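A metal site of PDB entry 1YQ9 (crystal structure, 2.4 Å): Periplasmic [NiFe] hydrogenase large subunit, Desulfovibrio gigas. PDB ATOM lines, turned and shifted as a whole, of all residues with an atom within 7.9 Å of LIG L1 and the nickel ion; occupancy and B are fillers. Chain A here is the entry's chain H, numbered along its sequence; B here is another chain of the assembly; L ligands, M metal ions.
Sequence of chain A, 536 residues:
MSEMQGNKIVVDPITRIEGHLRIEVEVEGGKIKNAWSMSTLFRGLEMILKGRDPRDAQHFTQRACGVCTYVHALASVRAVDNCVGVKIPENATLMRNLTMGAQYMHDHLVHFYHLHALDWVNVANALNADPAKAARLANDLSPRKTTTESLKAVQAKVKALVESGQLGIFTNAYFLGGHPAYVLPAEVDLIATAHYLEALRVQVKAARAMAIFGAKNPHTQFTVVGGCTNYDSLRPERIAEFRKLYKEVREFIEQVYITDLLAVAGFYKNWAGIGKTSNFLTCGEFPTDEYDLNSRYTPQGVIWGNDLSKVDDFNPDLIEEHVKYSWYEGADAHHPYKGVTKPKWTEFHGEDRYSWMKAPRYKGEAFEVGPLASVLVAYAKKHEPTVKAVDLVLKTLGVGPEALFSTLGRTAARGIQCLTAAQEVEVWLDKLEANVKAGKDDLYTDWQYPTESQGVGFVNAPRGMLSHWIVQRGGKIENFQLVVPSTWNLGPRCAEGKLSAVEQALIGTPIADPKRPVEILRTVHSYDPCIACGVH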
ATOM      1  N   GLU A  18      -2.368  -6.885   4.401  1.00  0.00           N
ATOM      2  CA  GLU A  18      -2.386  -8.281   4.839  1.00  0.00           C
ATOM      3  C   GLU A  18      -3.822  -8.751   4.866  1.00  0.00           C
ATOM      4  O   GLU A  18      -4.683  -8.085   5.443  1.00  0.00           O
ATOM      5  CB  GLU A  18      -1.763  -8.420   6.232  1.00  0.00           C
ATOM      6  CG  GLU A  18      -1.423  -9.843   6.613  1.00  0.00           C
ATOM      7  CD  GLU A  18      -2.653 -10.726   6.812  1.00  0.00           C
ATOM      8  OE1 GLU A  18      -3.674 -10.260   7.353  1.00  0.00           O
ATOM      9  OE2 GLU A  18      -2.595 -11.915   6.447  1.00  0.00           O
ATOM     10  N   GLN A  62       0.843 -15.998  18.119  1.00  0.00           N
ATOM     11  CA  GLN A  62       1.773 -15.370  17.181  1.00  0.00           C
ATOM     12  C   GLN A  62       1.300 -15.591  15.738  1.00  0.00           C
ATOM     13  O   GLN A  62       1.481 -14.725  14.870  1.00  0.00           O
ATOM     14  CB  GLN A  62       3.244 -15.806  17.344  1.00  0.00           C
ATOM     15  CG  GLN A  62       4.174 -14.885  16.511  1.00  0.00           C
ATOM     16  CD  GLN A  62       5.644 -14.978  16.869  1.00  0.00           C
ATOM     17  OE1 GLN A  62       6.381 -14.026  16.680  1.00  0.00           O
ATOM     18  NE2 GLN A  62       6.087 -16.140  17.359  1.00  0.00           N
ATOM     19  N   ALA A  64      -1.597 -15.463  14.606  1.00  0.00           N
ATOM     20  CA  ALA A  64      -2.622 -14.487  14.205  1.00  0.00           C
ATOM     21  C   ALA A  64      -2.162 -13.714  12.957  1.00  0.00           C
ATOM     22  O   ALA A  64      -2.982 -13.413  12.077  1.00  0.00           O
ATOM     23  CB  ALA A  64      -2.942 -13.527  15.331  1.00  0.00           C
ATOM     24  N   CYS A  65      -0.865 -13.403  12.896  1.00  0.00           N
ATOM     25  CA  CYS A  65      -0.333 -12.624  11.778  1.00  0.00           C
ATOM     26  C   CYS A  65       1.190 -12.691  11.641  1.00  0.00           C
ATOM     27  O   CYS A  65       1.930 -12.555  12.609  1.00  0.00           O
ATOM     28  CB  CYS A  65      -0.779 -11.168  11.887  1.00  0.00           C
ATOM     29  SG  CYS A  65      -0.384 -10.144  10.439  1.00  0.00           S
ATOM     30  N   GLY A  66       1.665 -12.893  10.413  1.00  0.00           N
ATOM     31  CA  GLY A  66       3.097 -12.957  10.155  1.00  0.00           C
ATOM     32  C   GLY A  66       3.725 -11.649   9.679  1.00  0.00           C
ATOM     33  O   GLY A  66       4.954 -11.572   9.489  1.00  0.00           O
ATOM     34  N   VAL A  67       2.879 -10.624   9.467  1.00  0.00           N
ATOM     35  CA  VAL A  67       3.377  -9.290   9.136  1.00  0.00           C
ATOM     36  C   VAL A  67       3.746  -8.522  10.406  1.00  0.00           C
ATOM     37  O   VAL A  67       4.875  -8.057  10.556  1.00  0.00           O
ATOM     38  CB  VAL A  67       2.359  -8.462   8.333  1.00  0.00           C
ATOM     39  CG1 VAL A  67       2.954  -7.079   8.022  1.00  0.00           C
ATOM     40  CG2 VAL A  67       1.996  -9.191   7.045  1.00  0.00           C
ATOM     41  N   CYS A  68       2.795  -8.372  11.330  1.00  0.00           N
ATOM     42  CA  CYS A  68       3.164  -7.932  12.659  1.00  0.00           C
ATOM     43  C   CYS A  68       3.555  -9.180  13.472  1.00  0.00           C
ATOM     44  O   CYS A  68       2.889  -9.561  14.417  1.00  0.00           O
ATOM     45  CB  CYS A  68       2.032  -7.136  13.316  1.00  0.00           C
ATOM     46  SG  CYS A  68       0.485  -8.046  13.483  1.00  0.00           S
ATOM     47  N   THR A  69       4.628  -9.839  13.047  1.00  0.00           N
ATOM     48  CA  THR A  69       5.133 -10.970  13.792  1.00  0.00           C
ATOM     49  C   THR A  69       5.661 -10.466  15.143  1.00  0.00           C
ATOM     50  O   THR A  69       5.905  -9.255  15.316  1.00  0.00           O
ATOM     51  CB  THR A  69       6.231 -11.702  12.959  1.00  0.00           C
ATOM     52  OG1 THR A  69       6.475 -13.011  13.503  1.00  0.00           O
ATOM     53  CG2 THR A  69       7.579 -10.972  13.056  1.00  0.00           C
ATOM     54  N   VAL A  71       4.539  -9.385  17.836  1.00  0.00           N
ATOM     55  CA  VAL A  71       3.637  -8.597  18.677  1.00  0.00           C
ATOM     56  C   VAL A  71       2.561  -9.416  19.424  1.00  0.00           C
ATOM     57  O   VAL A  71       2.283  -9.134  20.580  1.00  0.00           O
ATOM     58  CB  VAL A  71       3.031  -7.347  17.953  1.00  0.00           C
ATOM     59  CG1 VAL A  71       4.083  -6.674  17.093  1.00  0.00           C
ATOM     60  CG2 VAL A  71       1.774  -7.695  17.125  1.00  0.00           C
ATOM     61  N   HIS A  72       1.970 -10.425  18.778  1.00  0.00           N
ATOM     62  CA  HIS A  72       1.024 -11.281  19.509  1.00  0.00           C
ATOM     63  C   HIS A  72       1.712 -12.198  20.513  1.00  0.00           C
ATOM     64  O   HIS A  72       1.140 -12.516  21.551  1.00  0.00           O
ATOM     65  CB  HIS A  72       0.131 -12.101  18.573  1.00  0.00           C
ATOM     66  CG  HIS A  72      -0.871 -11.279  17.831  1.00  0.00           C
ATOM     67  ND1 HIS A  72      -2.110 -10.970  18.348  1.00  0.00           N
ATOM     68  CD2 HIS A  72      -0.801 -10.683  16.616  1.00  0.00           C
ATOM     69  CE1 HIS A  72      -2.764 -10.228  17.471  1.00  0.00           C
ATOM     70  NE2 HIS A  72      -1.996 -10.029  16.422  1.00  0.00           N
ATOM     71  N   GLN A 103      10.948  -4.298  15.179  1.00  0.00           N
ATOM     72  CA  GLN A 103       9.694  -4.527  14.458  1.00  0.00           C
ATOM     73  C   GLN A 103       9.083  -3.226  13.925  1.00  0.00           C
ATOM     74  O   GLN A 103       8.608  -3.174  12.792  1.00  0.00           O
ATOM     75  CB  GLN A 103       8.682  -5.260  15.349  1.00  0.00           C
ATOM     76  CG  GLN A 103       7.266  -5.377  14.730  1.00  0.00           C
ATOM     77  CD  GLN A 103       7.257  -6.252  13.489  1.00  0.00           C
ATOM     78  OE1 GLN A 103       8.135  -7.101  13.299  1.00  0.00           O
ATOM     79  NE2 GLN A 103       6.267  -6.050  12.620  1.00  0.00           N
ATOM     80  N   ASP A 107       8.528  -2.826  10.108  1.00  0.00           N
ATOM     81  CA  ASP A 107       7.140  -2.820   9.658  1.00  0.00           C
ATOM     82  C   ASP A 107       6.792  -1.532   8.896  1.00  0.00           C
ATOM     83  O   ASP A 107       6.200  -1.562   7.825  1.00  0.00           O
ATOM     84  CB  ASP A 107       6.197  -3.021  10.875  1.00  0.00           C
ATOM     85  CG  ASP A 107       4.858  -3.642  10.487  1.00  0.00           C
ATOM     86  OD1 ASP A 107       4.282  -4.421  11.303  1.00  0.00           O
ATOM     87  OD2 ASP A 107       4.295  -3.411   9.387  1.00  0.00           O
ATOM     88  N   ALA A 461       1.165  -2.130  19.141  1.00  0.00           N
ATOM     89  CA  ALA A 461       1.787  -2.671  17.941  1.00  0.00           C
ATOM     90  C   ALA A 461       1.892  -1.558  16.909  1.00  0.00           C
ATOM     91  O   ALA A 461       1.352  -0.458  17.111  1.00  0.00           O
ATOM     92  CB  ALA A 461       0.962  -3.851  17.414  1.00  0.00           C
ATOM     93  N   PRO A 462       2.598  -1.815  15.822  1.00  0.00           N
ATOM     94  CA  PRO A 462       2.735  -0.815  14.744  1.00  0.00           C
ATOM     95  C   PRO A 462       1.373  -0.335  14.191  1.00  0.00           C
ATOM     96  O   PRO A 462       1.268   0.793  13.689  1.00  0.00           O
ATOM     97  CB  PRO A 462       3.517  -1.585  13.672  1.00  0.00           C
ATOM     98  CG  PRO A 462       4.290  -2.597  14.469  1.00  0.00           C
ATOM     99  CD  PRO A 462       3.347  -3.061  15.537  1.00  0.00           C
ATOM    100  N   ARG A 463       0.346  -1.176  14.299  1.00  0.00           N
ATOM    101  CA  ARG A 463      -0.993  -0.791  13.868  1.00  0.00           C
ATOM    102  C   ARG A 463      -1.872  -0.241  14.991  1.00  0.00           C
ATOM    103  O   ARG A 463      -2.983   0.243  14.746  1.00  0.00           O
ATOM    104  CB  ARG A 463      -1.685  -1.961  13.132  1.00  0.00           C
ATOM    105  CG  ARG A 463      -1.261  -2.103  11.663  1.00  0.00           C
ATOM    106  CD  ARG A 463      -1.342  -3.522  11.044  1.00  0.00           C
ATOM    107  NE  ARG A 463      -0.540  -3.547   9.821  1.00  0.00           N
ATOM    108  CZ  ARG A 463       0.775  -3.781   9.787  1.00  0.00           C
ATOM    109  NH1 ARG A 463       1.426  -4.088  10.899  1.00  0.00           N
ATOM    110  NH2 ARG A 463       1.439  -3.748   8.636  1.00  0.00           N
ATOM    111  N   GLY A 464      -1.370  -0.277  16.237  1.00  0.00           N
ATOM    112  CA  GLY A 464      -2.134   0.273  17.365  1.00  0.00           C
ATOM    113  C   GLY A 464      -2.324  -0.598  18.613  1.00  0.00           C
ATOM    114  O   GLY A 464      -1.573  -1.534  18.866  1.00  0.00           O
ATOM    115  N   VAL A 484      -7.708  -6.579  18.616  1.00  0.00           N
ATOM    116  CA  VAL A 484      -6.485  -6.154  17.929  1.00  0.00           C
ATOM    117  C   VAL A 484      -6.698  -4.888  17.089  1.00  0.00           C
ATOM    118  O   VAL A 484      -7.833  -4.550  16.731  1.00  0.00           O
ATOM    119  CB  VAL A 484      -5.738  -7.382  17.261  1.00  0.00           C
ATOM    120  CG1 VAL A 484      -6.573  -8.678  17.358  1.00  0.00           C
ATOM    121  CG2 VAL A 484      -5.253  -7.092  15.864  1.00  0.00           C
ATOM    122  N   PRO A 485      -5.634  -4.115  16.875  1.00  0.00           N
ATOM    123  CA  PRO A 485      -5.769  -2.754  16.314  1.00  0.00           C
ATOM    124  C   PRO A 485      -6.635  -2.673  15.058  1.00  0.00           C
ATOM    125  O   PRO A 485      -7.492  -1.813  14.956  1.00  0.00           O
ATOM    126  CB  PRO A 485      -4.317  -2.287  16.057  1.00  0.00           C
ATOM    127  CG  PRO A 485      -3.419  -3.483  16.384  1.00  0.00           C
ATOM    128  CD  PRO A 485      -4.242  -4.449  17.226  1.00  0.00           C
ATOM    129  N   SER A 486      -6.428  -3.577  14.108  1.00  0.00           N
ATOM    130  CA  SER A 486      -7.265  -3.582  12.920  1.00  0.00           C
ATOM    131  C   SER A 486      -8.703  -3.968  13.241  1.00  0.00           C
ATOM    132  O   SER A 486      -9.606  -3.635  12.485  1.00  0.00           O
ATOM    133  CB  SER A 486      -6.697  -4.516  11.842  1.00  0.00           C
ATOM    134  OG  SER A 486      -5.408  -4.110  11.422  1.00  0.00           O
ATOM    135  N   ASP A 528      -3.136   1.012   7.314  1.00  0.00           N
ATOM    136  CA  ASP A 528      -2.286  -0.177   7.319  1.00  0.00           C
ATOM    137  C   ASP A 528      -3.070  -1.421   7.751  1.00  0.00           C
ATOM    138  O   ASP A 528      -2.722  -2.064   8.737  1.00  0.00           O
ATOM    139  CB  ASP A 528      -1.119   0.049   8.274  1.00  0.00           C
ATOM    140  CG  ASP A 528      -0.031  -1.003   8.166  1.00  0.00           C
ATOM    141  OD1 ASP A 528       0.986  -0.850   8.881  1.00  0.00           O
ATOM    142  OD2 ASP A 528      -0.074  -2.008   7.404  1.00  0.00           O
ATOM    143  N   PRO A 529      -4.113  -1.784   6.996  1.00  0.00           N
ATOM    144  CA  PRO A 529      -5.018  -2.872   7.415  1.00  0.00           C
ATOM    145  C   PRO A 529      -4.347  -4.237   7.512  1.00  0.00           C
ATOM    146  O   PRO A 529      -3.493  -4.582   6.685  1.00  0.00           O
ATOM    147  CB  PRO A 529      -6.093  -2.880   6.308  1.00  0.00           C
ATOM    148  CG  PRO A 529      -5.971  -1.537   5.662  1.00  0.00           C
ATOM    149  CD  PRO A 529      -4.507  -1.224   5.694  1.00  0.00           C
ATOM    150  N   CYS A 530      -4.731  -5.016   8.525  1.00  0.00           N
ATOM    151  CA  CYS A 530      -4.303  -6.411   8.638  1.00  0.00           C
ATOM    152  C   CYS A 530      -5.521  -7.261   9.016  1.00  0.00           C
ATOM    153  O   CYS A 530      -5.999  -7.199  10.139  1.00  0.00           O
ATOM    154  CB  CYS A 530      -3.197  -6.557   9.693  1.00  0.00           C
ATOM    155  SG  CYS A 530      -2.414  -8.202   9.763  1.00  0.00           S
ATOM    156  N   ILE A 531      -6.016  -8.055   8.069  1.00  0.00           N
ATOM    157  CA  ILE A 531      -7.280  -8.742   8.271  1.00  0.00           C
ATOM    158  C   ILE A 531      -7.111 -10.058   9.056  1.00  0.00           C
ATOM    159  O   ILE A 531      -8.035 -10.517   9.741  1.00  0.00           O
ATOM    160  CB  ILE A 531      -8.031  -8.946   6.918  1.00  0.00           C
ATOM    161  CG1 ILE A 531      -8.050  -7.644   6.112  1.00  0.00           C
ATOM    162  CG2 ILE A 531      -9.475  -9.440   7.161  1.00  0.00           C
ATOM    163  CD1 ILE A 531      -8.535  -6.453   6.921  1.00  0.00           C
ATOM    164  N   ALA A 532      -5.942 -10.676   8.982  1.00  0.00           N
ATOM    165  CA  ALA A 532      -5.706 -11.848   9.801  1.00  0.00           C
ATOM    166  C   ALA A 532      -5.640 -11.424  11.279  1.00  0.00           C
ATOM    167  O   ALA A 532      -6.206 -12.097  12.149  1.00  0.00           O
ATOM    168  CB  ALA A 532      -4.465 -12.568   9.384  1.00  0.00           C
ATOM    169  N   CYS A 533      -4.940 -10.308  11.541  1.00  0.00           N
ATOM    170  CA  CYS A 533      -4.982  -9.664  12.850  1.00  0.00           C
ATOM    171  C   CYS A 533      -6.411  -9.347  13.307  1.00  0.00           C
ATOM    172  O   CYS A 533      -6.826  -9.752  14.391  1.00  0.00           O
ATOM    173  CB  CYS A 533      -4.165  -8.362  12.850  1.00  0.00           C
ATOM    174  SG  CYS A 533      -2.459  -8.566  13.402  1.00  0.00           S
ATOM    175  N   GLY A 534      -7.148  -8.624  12.466  1.00  0.00           N
ATOM    176  CA  GLY A 534      -8.459  -8.122  12.873  1.00  0.00           C
ATOM    177  C   GLY A 534      -9.470  -9.190  13.237  1.00  0.00           C
ATOM    178  O   GLY A 534     -10.263  -8.993  14.174  1.00  0.00           O
ATOM    179  N   CYS B  17      -1.562 -16.421   7.584  1.00  0.00           N
ATOM    180  CA  CYS B  17      -1.178 -15.246   8.367  1.00  0.00           C
ATOM    181  C   CYS B  17      -0.248 -14.363   7.573  1.00  0.00           C
ATOM    182  O   CYS B  17       0.139 -13.310   8.022  1.00  0.00           O
ATOM    183  CB  CYS B  17      -0.503 -15.656   9.696  1.00  0.00           C
ATOM    184  SG  CYS B  17       1.235 -16.172   9.555  1.00  0.00           S
ATOM    185  N   THR B  18       0.139 -14.813   6.383  1.00  0.00           N
ATOM    186  CA  THR B  18       1.027 -14.040   5.497  1.00  0.00           C
ATOM    187  C   THR B  18       2.498 -14.074   5.947  1.00  0.00           C
ATOM    188  O   THR B  18       3.353 -13.396   5.374  1.00  0.00           O
ATOM    189  CB  THR B  18       0.518 -12.582   5.353  1.00  0.00           C
ATOM    190  OG1 THR B  18      -0.847 -12.571   4.911  1.00  0.00           O
ATOM    191  CG2 THR B  18       1.276 -11.850   4.224  1.00  0.00           C
ATOM    192  N   GLU B  22       5.961 -13.096   3.776  1.00  0.00           N
ATOM    193  CA  GLU B  22       7.061 -12.366   4.418  1.00  0.00           C
ATOM    194  C   GLU B  22       8.380 -13.137   4.396  1.00  0.00           C
ATOM    195  O   GLU B  22       9.440 -12.526   4.235  1.00  0.00           O
ATOM    196  CB  GLU B  22       6.726 -11.936   5.855  1.00  0.00           C
ATOM    197  CG  GLU B  22       5.640 -10.864   5.971  1.00  0.00           C
ATOM    198  CD  GLU B  22       6.152  -9.425   5.828  1.00  0.00           C
ATOM    199  OE1 GLU B  22       5.284  -8.536   5.686  1.00  0.00           O
ATOM    200  OE2 GLU B  22       7.394  -9.154   5.876  1.00  0.00           O
HETATM  201  O1  LIG L   1      -0.773  -6.452  11.977  1.00  0.00           O
HETATM  202  O2  LIG L   1      -0.012  -6.536  10.749  1.00  0.00           O
HETATM  203 FE1  LG2 L   2      -1.284  -6.584  13.785  1.00  0.00          FE
HETATM  204  C1  LG2 L   2      -2.840  -5.535  13.496  1.00  0.00           C
HETATM  205  N1  LG2 L   2      -3.785  -4.887  13.268  1.00  0.00           N
HETATM  206  C2  LG2 L   2      -0.192  -5.030  13.959  1.00  0.00           C
HETATM  207  N2  LG2 L   2       0.485  -4.098  14.068  1.00  0.00           N
HETATM  208  C3  LG2 L   2      -1.513  -6.569  15.496  1.00  0.00           C
HETATM  209  O1  LG2 L   2      -1.630  -6.551  16.654  1.00  0.00           O
HETATM  210 NI    NI M   1      -0.847  -8.229  11.357  1.00  0.00          NI
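A nitrogen (N2) of LG2 L2 is in hydrogen-bond range of the backbone NH of Arg 463 (2.9 Å).
N of Cys 68 sits close to O2 of LIG L1 (3.4 Å).
N2 of LG2 L2 lies close to NH1 of Arg 463 (3.3 Å).
N of Ser 486 lies within hydrogen-bond range of N1 of LG2 L2 (3.1 Å).
The side-chain sulfur (SG) of Cys 68 binds an iron atom (FE1) of LG2 L2 (2.3 Å).
A nitrogen (N1) of LG2 L2 is in hydrogen-bond range of the side-chain hydroxyl of Ser 486, 2.6 Å away.
FE1 of LG2 L2 is bound by SG of Cys 533 (2.3 Å).
NH1 of Arg 463 sits close to O2 of LIG L1 (2.8 Å).
O1 of LIG L1 binds FE1 of LG2 L2 (1.9 Å).
The side-chain sulfur of Cys 530 sits close to the side-chain carboxylate of Glu 18 of chain A (3.4 Å).
The backbone carbonyl oxygen (O) of Val 67 sits at hydrogen-bond distance from the side-chain amide nitrogen (NE2) of Gln 103, 3.2 Å away.
NH1 of Arg 463 lies within salt-bridge range of OD1 of Asp 107, 2.9 Å away.
A ring nitrogen (NE2) of His 72 sits close to the side-chain sulfur (SG) of Cys 533 (3.4 Å).
N of Cys 530 lies within hydrogen-bond range of OG of Ser 486 (3.1 Å).
The side-chain carboxylate (OD2) of Asp 528 is in salt-bridge range of the guanidinium group (NH2) of Arg 463.
SG of Cys 65 sits close to N of Val 67, 3.4 Å away.
Val 67 touches LIG L1.
Hydrophobic or aromatic side chains within 4 Å of LIG L1: Val 67.
Within 4 Å of LIG L1: Cys 65, Val 67, Cys 68, Arg 463, Cys 530 and Cys 533.
The nearest printed residue that does not touch the nickel ion is Val 67 (4.4 Å).
An oxygen (O1) of LIG L1 is bound to the nickel ion, at 1.9 Å.
SG of Cys 65 binds the nickel ion (2.2 Å).
The nickel ion is bound by the side-chain sulfur (SG) of Cys 530 (2.2 Å).
The nickel ion is bound by SG of Cys 68 (2.5 Å).
The nickel ion is bound by SG of Cys 533.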
